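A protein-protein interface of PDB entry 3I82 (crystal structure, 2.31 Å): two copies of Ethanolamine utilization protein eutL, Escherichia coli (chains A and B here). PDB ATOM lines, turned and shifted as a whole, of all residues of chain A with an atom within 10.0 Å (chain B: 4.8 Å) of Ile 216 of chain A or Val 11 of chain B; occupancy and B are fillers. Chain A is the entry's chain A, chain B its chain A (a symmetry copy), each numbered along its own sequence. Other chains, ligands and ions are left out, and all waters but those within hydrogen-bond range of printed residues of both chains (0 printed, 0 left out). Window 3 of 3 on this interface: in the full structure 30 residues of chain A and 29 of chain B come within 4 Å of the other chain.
The backbone NH (N) of Thr 12 of chain B lies within hydrogen-bond range of the backbone carbonyl oxygen (O) of Ser 41 of chain B.
The backbone carbonyl oxygen (O) of Ala 13 of chain B sits at hydrogen-bond distance from the backbone NH (N) of Ser 41 of chain B (2.9 Å).
No position is printed for both chains.
Of the 14 pairs that touch across the chains among the printed residues, none has its exchanged pair printed and touching as well.
The guanidinium group (NH2) of Arg 15 of chain B is in hydrogen-bond range of the backbone carbonyl oxygen (O) of Asn 214 of chain A (2.9 Å).
The backbone carbonyl oxygen (O) of Pro 215 of chain A is in hydrogen-bond range of the backbone NH (N) of Met 14 of chain B, 2.8 Å away.
The side-chain amide nitrogen of Gln 217 of chain A sits close to the guanidinium group of Arg 15 of chain B (3.4 Å).
O of Glu 210 of chain A sits at hydrogen-bond distance from NH2 of Arg 15 of chain B (3.3 Å).
The backbone carbonyl oxygen (O) of Pro 215 of chain A sits at hydrogen-bond distance from the guanidinium group (NH1) of Arg 15 of chain B (3.3 Å).
Printed residues of chain B within 4 Å of Glu 210 of chain A: Arg 15.
Arg 213 of chain A touches none of the printed residues of chain B.
Of the printed residues of chain B, Ile 216 of chain A touches Val 11 and Ala 13.
Of the printed residues of chain B, Gln 217 of chain A touches Arg 15.
Pro 9 of chain B touches none of the printed residues of chain A.
No residue of chain A comes within 4 Å of Ser 10 of chain B.
Of chain A, only Ile 216 comes within 4 Å of Val 11 of chain B.
Thr 12 of chain B touches just one residue of chain A: Pro 215.
Of chain A, only Leu 156 (3.9 Å) and Pro 215 (2.8 Å) come within 4 Å of Met 14 of chain B.
Printed residues of chain A within 4 Å of Ile 40 of chain B: Leu 156 (3.6 Å).
Of the printed residues of chain A, Ser 41 of chain B touches Leu 156 (3.8 Å).
Ile 104 of chain B touches none of the printed residues of chain A.
Ala 13 of chain B touches Leu 156 of chain A (O to CD1, 3.5 Å).
Leu 156 of chain A touches Met 14 of chain B (CD1 to N, 3.9 Å).
Ile 40 of chain B touches Leu 156 of chain A (N to CD1, 3.6 Å).
Leu 156 of chain A touches Ser 41 of chain B.
Arg 15 of chain B touches Ile 211 of chain A.
Pro 215 of chain A touches Thr 12 of chain B.
Ala 13 of chain B touches Pro 215 of chain A (CA to O, 3.3 Å).
Ile 216 of chain A touches Val 11 of chain B (CD1 to O, 3.1 Å).
Ala 13 of chain B touches Ile 216 of chain A.
Printed residues of chain B that touch a printed residue of chain A: Val 11, Thr 12, Ala 13, Met 14, Arg 15, Ile 40 and Ser 41.
Hydrophobic or aromatic side chains of chain A that line the printed part of chain B: Leu 156, Ile 211, Pro 215 and Ile 216.
Along chain A the printed residues that touch a printed residue of chain B span positions 156 to 217.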
ATOM      1  N   LEU A 156     -24.082   0.180   2.833  1.00  0.00           N
ATOM      2  CA  LEU A 156     -22.662   0.347   3.157  1.00  0.00           C
ATOM      3  C   LEU A 156     -21.733  -0.529   2.314  1.00  0.00           C
ATOM      4  O   LEU A 156     -20.699  -0.063   1.834  1.00  0.00           O
ATOM      5  CB  LEU A 156     -22.411   0.114   4.657  1.00  0.00           C
ATOM      6  CG  LEU A 156     -21.097   0.709   5.196  1.00  0.00           C
ATOM      7  CD1 LEU A 156     -21.224   1.080   6.664  1.00  0.00           C
ATOM      8  CD2 LEU A 156     -19.944  -0.258   4.975  1.00  0.00           C
ATOM      9  N   GLU A 157     -22.103  -1.796   2.162  1.00  0.00           N
ATOM     10  CA  GLU A 157     -21.340  -2.753   1.363  1.00  0.00           C
ATOM     11  C   GLU A 157     -21.192  -2.200  -0.048  1.00  0.00           C
ATOM     12  O   GLU A 157     -20.106  -2.232  -0.625  1.00  0.00           O
ATOM     13  CB  GLU A 157     -22.057  -4.117   1.301  1.00  0.00           C
ATOM     14  CG  GLU A 157     -21.851  -5.047   2.515  1.00  0.00           C
ATOM     15  CD  GLU A 157     -22.833  -4.803   3.657  1.00  0.00           C
ATOM     16  OE1 GLU A 157     -23.268  -3.635   3.813  1.00  0.00           O
ATOM     17  OE2 GLU A 157     -23.127  -5.773   4.393  1.00  0.00           O
ATOM     18  N   LEU A 209     -17.581  -9.192   0.788  1.00  0.00           N
ATOM     19  CA  LEU A 209     -17.244 -10.331   1.645  1.00  0.00           C
ATOM     20  C   LEU A 209     -16.491  -9.855   2.891  1.00  0.00           C
ATOM     21  O   LEU A 209     -16.771 -10.327   3.990  1.00  0.00           O
ATOM     22  CB  LEU A 209     -16.404 -11.365   0.887  1.00  0.00           C
ATOM     23  CG  LEU A 209     -17.082 -12.200  -0.202  1.00  0.00           C
ATOM     24  CD1 LEU A 209     -16.029 -13.010  -0.954  1.00  0.00           C
ATOM     25  CD2 LEU A 209     -18.131 -13.127   0.377  1.00  0.00           C
ATOM     26  N   GLU A 210     -15.554  -8.924   2.711  1.00  0.00           N
ATOM     27  CA  GLU A 210     -14.779  -8.371   3.831  1.00  0.00           C
ATOM     28  C   GLU A 210     -15.696  -7.797   4.900  1.00  0.00           C
ATOM     29  O   GLU A 210     -15.519  -8.057   6.094  1.00  0.00           O
ATOM     30  CB  GLU A 210     -13.827  -7.276   3.347  1.00  0.00           C
ATOM     31  CG  GLU A 210     -12.542  -7.812   2.757  1.00  0.00           C
ATOM     32  CD  GLU A 210     -11.699  -6.736   2.103  1.00  0.00           C
ATOM     33  OE1 GLU A 210     -11.559  -5.648   2.704  1.00  0.00           O
ATOM     34  OE2 GLU A 210     -11.169  -6.984   0.993  1.00  0.00           O
ATOM     35  N   ILE A 211     -16.670  -7.005   4.468  1.00  0.00           N
ATOM     36  CA  ILE A 211     -17.625  -6.417   5.399  1.00  0.00           C
ATOM     37  C   ILE A 211     -18.497  -7.521   6.009  1.00  0.00           C
ATOM     38  O   ILE A 211     -18.867  -7.461   7.181  1.00  0.00           O
ATOM     39  CB  ILE A 211     -18.482  -5.345   4.695  1.00  0.00           C
ATOM     40  CG1 ILE A 211     -17.581  -4.184   4.262  1.00  0.00           C
ATOM     41  CG2 ILE A 211     -19.589  -4.843   5.615  1.00  0.00           C
ATOM     42  CD1 ILE A 211     -18.268  -3.146   3.410  1.00  0.00           C
ATOM     43  N   ALA A 212     -18.810  -8.542   5.218  1.00  0.00           N
ATOM     44  CA  ALA A 212     -19.598  -9.671   5.711  1.00  0.00           C
ATOM     45  C   ALA A 212     -18.882 -10.391   6.857  1.00  0.00           C
ATOM     46  O   ALA A 212     -19.514 -10.785   7.835  1.00  0.00           O
ATOM     47  CB  ALA A 212     -19.884 -10.644   4.576  1.00  0.00           C
ATOM     48  N   ARG A 213     -17.569 -10.558   6.733  1.00  0.00           N
ATOM     49  CA  ARG A 213     -16.769 -11.228   7.758  1.00  0.00           C
ATOM     50  C   ARG A 213     -16.592 -10.356   9.016  1.00  0.00           C
ATOM     51  O   ARG A 213     -16.808 -10.819  10.133  1.00  0.00           O
ATOM     52  CB  ARG A 213     -15.398 -11.618   7.190  1.00  0.00           C
ATOM     53  CG  ARG A 213     -15.427 -12.815   6.230  1.00  0.00           C
ATOM     54  CD  ARG A 213     -14.017 -13.325   5.913  1.00  0.00           C
ATOM     55  NE  ARG A 213     -13.318 -12.477   4.947  1.00  0.00           N
ATOM     56  CZ  ARG A 213     -13.379 -12.627   3.626  1.00  0.00           C
ATOM     57  NH1 ARG A 213     -14.103 -13.606   3.088  1.00  0.00           N
ATOM     58  NH2 ARG A 213     -12.719 -11.790   2.833  1.00  0.00           N
ATOM     59  N   ASN A 214     -16.192  -9.101   8.826  1.00  0.00           N
ATOM     60  CA  ASN A 214     -16.002  -8.166   9.927  1.00  0.00           C
ATOM     61  C   ASN A 214     -16.751  -6.861   9.660  1.00  0.00           C
ATOM     62  O   ASN A 214     -16.154  -5.874   9.228  1.00  0.00           O
ATOM     63  CB  ASN A 214     -14.507  -7.876  10.113  1.00  0.00           C
ATOM     64  CG  ASN A 214     -13.744  -9.072  10.627  1.00  0.00           C
ATOM     65  OD1 ASN A 214     -13.829  -9.415  11.808  1.00  0.00           O
ATOM     66  ND2 ASN A 214     -12.992  -9.719   9.744  1.00  0.00           N
ATOM     67  N   PRO A 215     -18.065  -6.839   9.916  1.00  0.00           N
ATOM     68  CA  PRO A 215     -18.853  -5.641   9.629  1.00  0.00           C
ATOM     69  C   PRO A 215     -18.440  -4.402  10.422  1.00  0.00           C
ATOM     70  O   PRO A 215     -18.608  -3.284   9.915  1.00  0.00           O
ATOM     71  CB  PRO A 215     -20.286  -6.074   9.956  1.00  0.00           C
ATOM     72  CG  PRO A 215     -20.101  -7.100  11.011  1.00  0.00           C
ATOM     73  CD  PRO A 215     -18.903  -7.881  10.533  1.00  0.00           C
ATOM     74  N   ILE A 216     -17.920  -4.574  11.633  1.00  0.00           N
ATOM     75  CA  ILE A 216     -17.474  -3.429  12.416  1.00  0.00           C
ATOM     76  C   ILE A 216     -16.009  -3.611  12.823  1.00  0.00           C
ATOM     77  O   ILE A 216     -15.686  -4.456  13.676  1.00  0.00           O
ATOM     78  CB  ILE A 216     -18.323  -3.221  13.687  1.00  0.00           C
ATOM     79  CG1 ILE A 216     -19.799  -3.097  13.326  1.00  0.00           C
ATOM     80  CG2 ILE A 216     -17.865  -1.956  14.428  1.00  0.00           C
ATOM     81  CD1 ILE A 216     -20.717  -2.999  14.513  1.00  0.00           C
ATOM     82  N   GLN A 217     -15.127  -2.828  12.209  1.00  0.00           N
ATOM     83  CA  GLN A 217     -13.695  -2.927  12.501  1.00  0.00           C
ATOM     84  C   GLN A 217     -13.265  -2.031  13.662  1.00  0.00           C
ATOM     85  O   GLN A 217     -12.071  -2.025  14.017  1.00  0.00           O
ATOM     86  CB  GLN A 217     -12.874  -2.603  11.250  1.00  0.00           C
ATOM     87  CG  GLN A 217     -12.781  -3.764  10.270  1.00  0.00           C
ATOM     88  CD  GLN A 217     -11.825  -3.502   9.120  1.00  0.00           C
ATOM     89  OE1 GLN A 217     -11.096  -4.400   8.693  1.00  0.00           O
ATOM     90  NE2 GLN A 217     -11.828  -2.273   8.605  1.00  0.00           N
ATOM     91  N   PRO B   9     -30.117   1.240  20.623  1.00  0.00           N
ATOM     92  CA  PRO B   9     -29.743   0.951  19.250  1.00  0.00           C
ATOM     93  C   PRO B   9     -28.303   0.491  19.150  1.00  0.00           C
ATOM     94  O   PRO B   9     -27.522   0.632  20.095  1.00  0.00           O
ATOM     95  CB  PRO B   9     -29.981   2.280  18.534  1.00  0.00           C
ATOM     96  CG  PRO B   9     -29.765   3.309  19.577  1.00  0.00           C
ATOM     97  CD  PRO B   9     -30.020   2.679  20.925  1.00  0.00           C
ATOM     98  N   SER B  10     -27.963  -0.083  18.010  1.00  0.00           N
ATOM     99  CA  SER B  10     -26.620  -0.588  17.811  1.00  0.00           C
ATOM    100  C   SER B  10     -26.123  -0.305  16.418  1.00  0.00           C
ATOM    101  O   SER B  10     -26.903  -0.255  15.458  1.00  0.00           O
ATOM    102  CB  SER B  10     -26.579  -2.095  18.062  1.00  0.00           C
ATOM    103  OG  SER B  10     -27.694  -2.738  17.465  1.00  0.00           O
ATOM    104  N   VAL B  11     -24.803  -0.153  16.319  1.00  0.00           N
ATOM    105  CA  VAL B  11     -24.136   0.042  15.038  1.00  0.00           C
ATOM    106  C   VAL B  11     -24.067  -1.336  14.376  1.00  0.00           C
ATOM    107  O   VAL B  11     -23.674  -2.320  15.006  1.00  0.00           O
ATOM    108  CB  VAL B  11     -22.716   0.612  15.228  1.00  0.00           C
ATOM    109  CG1 VAL B  11     -22.020   0.780  13.877  1.00  0.00           C
ATOM    110  CG2 VAL B  11     -22.784   1.940  15.976  1.00  0.00           C
ATOM    111  N   THR B  12     -24.467  -1.410  13.112  1.00  0.00           N
ATOM    112  CA  THR B  12     -24.495  -2.679  12.387  1.00  0.00           C
ATOM    113  C   THR B  12     -23.347  -2.889  11.392  1.00  0.00           C
ATOM    114  O   THR B  12     -23.013  -4.029  11.070  1.00  0.00           O
ATOM    115  CB  THR B  12     -25.829  -2.852  11.645  1.00  0.00           C
ATOM    116  OG1 THR B  12     -26.083  -1.702  10.827  1.00  0.00           O
ATOM    117  CG2 THR B  12     -26.971  -3.049  12.641  1.00  0.00           C
ATOM    118  N   ALA B  13     -22.759  -1.809  10.893  1.00  0.00           N
ATOM    119  CA  ALA B  13     -21.628  -1.930   9.983  1.00  0.00           C
ATOM    120  C   ALA B  13     -20.854  -0.621   9.940  1.00  0.00           C
ATOM    121  O   ALA B  13     -21.438   0.446  10.117  1.00  0.00           O
ATOM    122  CB  ALA B  13     -22.107  -2.309   8.587  1.00  0.00           C
ATOM    123  N   MET B  14     -19.552  -0.695   9.685  1.00  0.00           N
ATOM    124  CA  MET B  14     -18.733   0.515   9.629  1.00  0.00           C
ATOM    125  C   MET B  14     -17.446   0.327   8.840  1.00  0.00           C
ATOM    126  O   MET B  14     -16.820  -0.734   8.893  1.00  0.00           O
ATOM    127  CB  MET B  14     -18.402   0.994  11.051  1.00  0.00           C
ATOM    128  CG  MET B  14     -17.579   2.278  11.104  1.00  0.00           C
ATOM    129  SD  MET B  14     -17.293   2.876  12.780  1.00  0.00           S
ATOM    130  CE  MET B  14     -15.918   1.820  13.282  1.00  0.00           C
ATOM    131  N   ARG B  15     -17.052   1.373   8.115  1.00  0.00           N
ATOM    132  CA  ARG B  15     -15.805   1.353   7.335  1.00  0.00           C
ATOM    133  C   ARG B  15     -15.289   2.760   7.091  1.00  0.00           C
ATOM    134  O   ARG B  15     -16.043   3.730   7.149  1.00  0.00           O
ATOM    135  CB  ARG B  15     -16.000   0.657   5.976  1.00  0.00           C
ATOM    136  CG  ARG B  15     -15.891  -0.867   5.998  1.00  0.00           C
ATOM    137  CD  ARG B  15     -14.508  -1.312   6.483  1.00  0.00           C
ATOM    138  NE  ARG B  15     -14.310  -2.758   6.382  1.00  0.00           N
ATOM    139  CZ  ARG B  15     -14.950  -3.667   7.117  1.00  0.00           C
ATOM    140  NH1 ARG B  15     -15.863  -3.294   8.006  1.00  0.00           N
ATOM    141  NH2 ARG B  15     -14.689  -4.958   6.939  1.00  0.00           N
ATOM    142  N   ILE B  40     -21.112   4.495   7.943  1.00  0.00           N
ATOM    143  CA  ILE B  40     -21.644   3.794   9.095  1.00  0.00           C
ATOM    144  C   ILE B  40     -23.131   3.514   8.953  1.00  0.00           C
ATOM    145  O   ILE B  40     -23.915   4.346   8.472  1.00  0.00           O
ATOM    146  CB  ILE B  40     -21.377   4.575  10.396  1.00  0.00           C
ATOM    147  CG1 ILE B  40     -21.788   3.728  11.608  1.00  0.00           C
ATOM    148  CG2 ILE B  40     -22.081   5.931  10.357  1.00  0.00           C
ATOM    149  CD1 ILE B  40     -21.266   4.266  12.944  1.00  0.00           C
ATOM    150  N   SER B  41     -23.527   2.318   9.369  1.00  0.00           N
ATOM    151  CA  SER B  41     -24.936   1.951   9.328  1.00  0.00           C
ATOM    152  C   SER B  41     -25.420   1.471  10.698  1.00  0.00           C
ATOM    153  O   SER B  41     -24.703   0.778  11.419  1.00  0.00           O
ATOM    154  CB  SER B  41     -25.176   0.874   8.270  1.00  0.00           C
ATOM    155  OG  SER B  41     -24.351  -0.261   8.469  1.00  0.00           O
ATOM    156  N   ALA B  42     -26.650   1.819  11.065  1.00  0.00           N
ATOM    157  CA  ALA B  42     -27.182   1.430  12.375  1.00  0.00           C
ATOM    158  C   ALA B  42     -28.637   1.006  12.283  1.00  0.00           C
ATOM    159  O   ALA B  42     -29.284   1.253  11.268  1.00  0.00           O
ATOM    160  CB  ALA B  42     -27.040   2.587  13.349  1.00  0.00           C
ATOM    161  N   ILE B 104     -20.439   6.506  17.237  1.00  0.00           N
ATOM    162  CA  ILE B 104     -20.626   5.256  17.967  1.00  0.00           C
ATOM    163  C   ILE B 104     -21.094   5.544  19.395  1.00  0.00           C
ATOM    164  O   ILE B 104     -22.104   4.996  19.842  1.00  0.00           O
ATOM    165  CB  ILE B 104     -19.321   4.426  18.041  1.00  0.00           C
ATOM    166  CG1 ILE B 104     -18.870   4.012  16.637  1.00  0.00           C
ATOM    167  CG2 ILE B 104     -19.536   3.179  18.905  1.00  0.00           C
ATOM    168  CD1 ILE B 104     -17.493   3.390  16.601  1.00  0.00           C
ATOM    169  N   ILE B 107     -24.599   6.707  19.499  1.00  0.00           N
ATOM    170  CA  ILE B 107     -25.594   5.744  19.031  1.00  0.00           C
ATOM    171  C   ILE B 107     -25.832   4.708  20.130  1.00  0.00           C
ATOM    172  O   ILE B 107     -26.946   4.227  20.313  1.00  0.00           O
ATOM    173  CB  ILE B 107     -25.153   5.045  17.733  1.00  0.00           C
ATOM    174  CG1 ILE B 107     -25.263   6.015  16.554  1.00  0.00           C
ATOM    175  CG2 ILE B 107     -26.017   3.830  17.456  1.00  0.00           C
ATOM    176  CD1 ILE B 107     -24.581   5.513  15.283  1.00  0.00           C
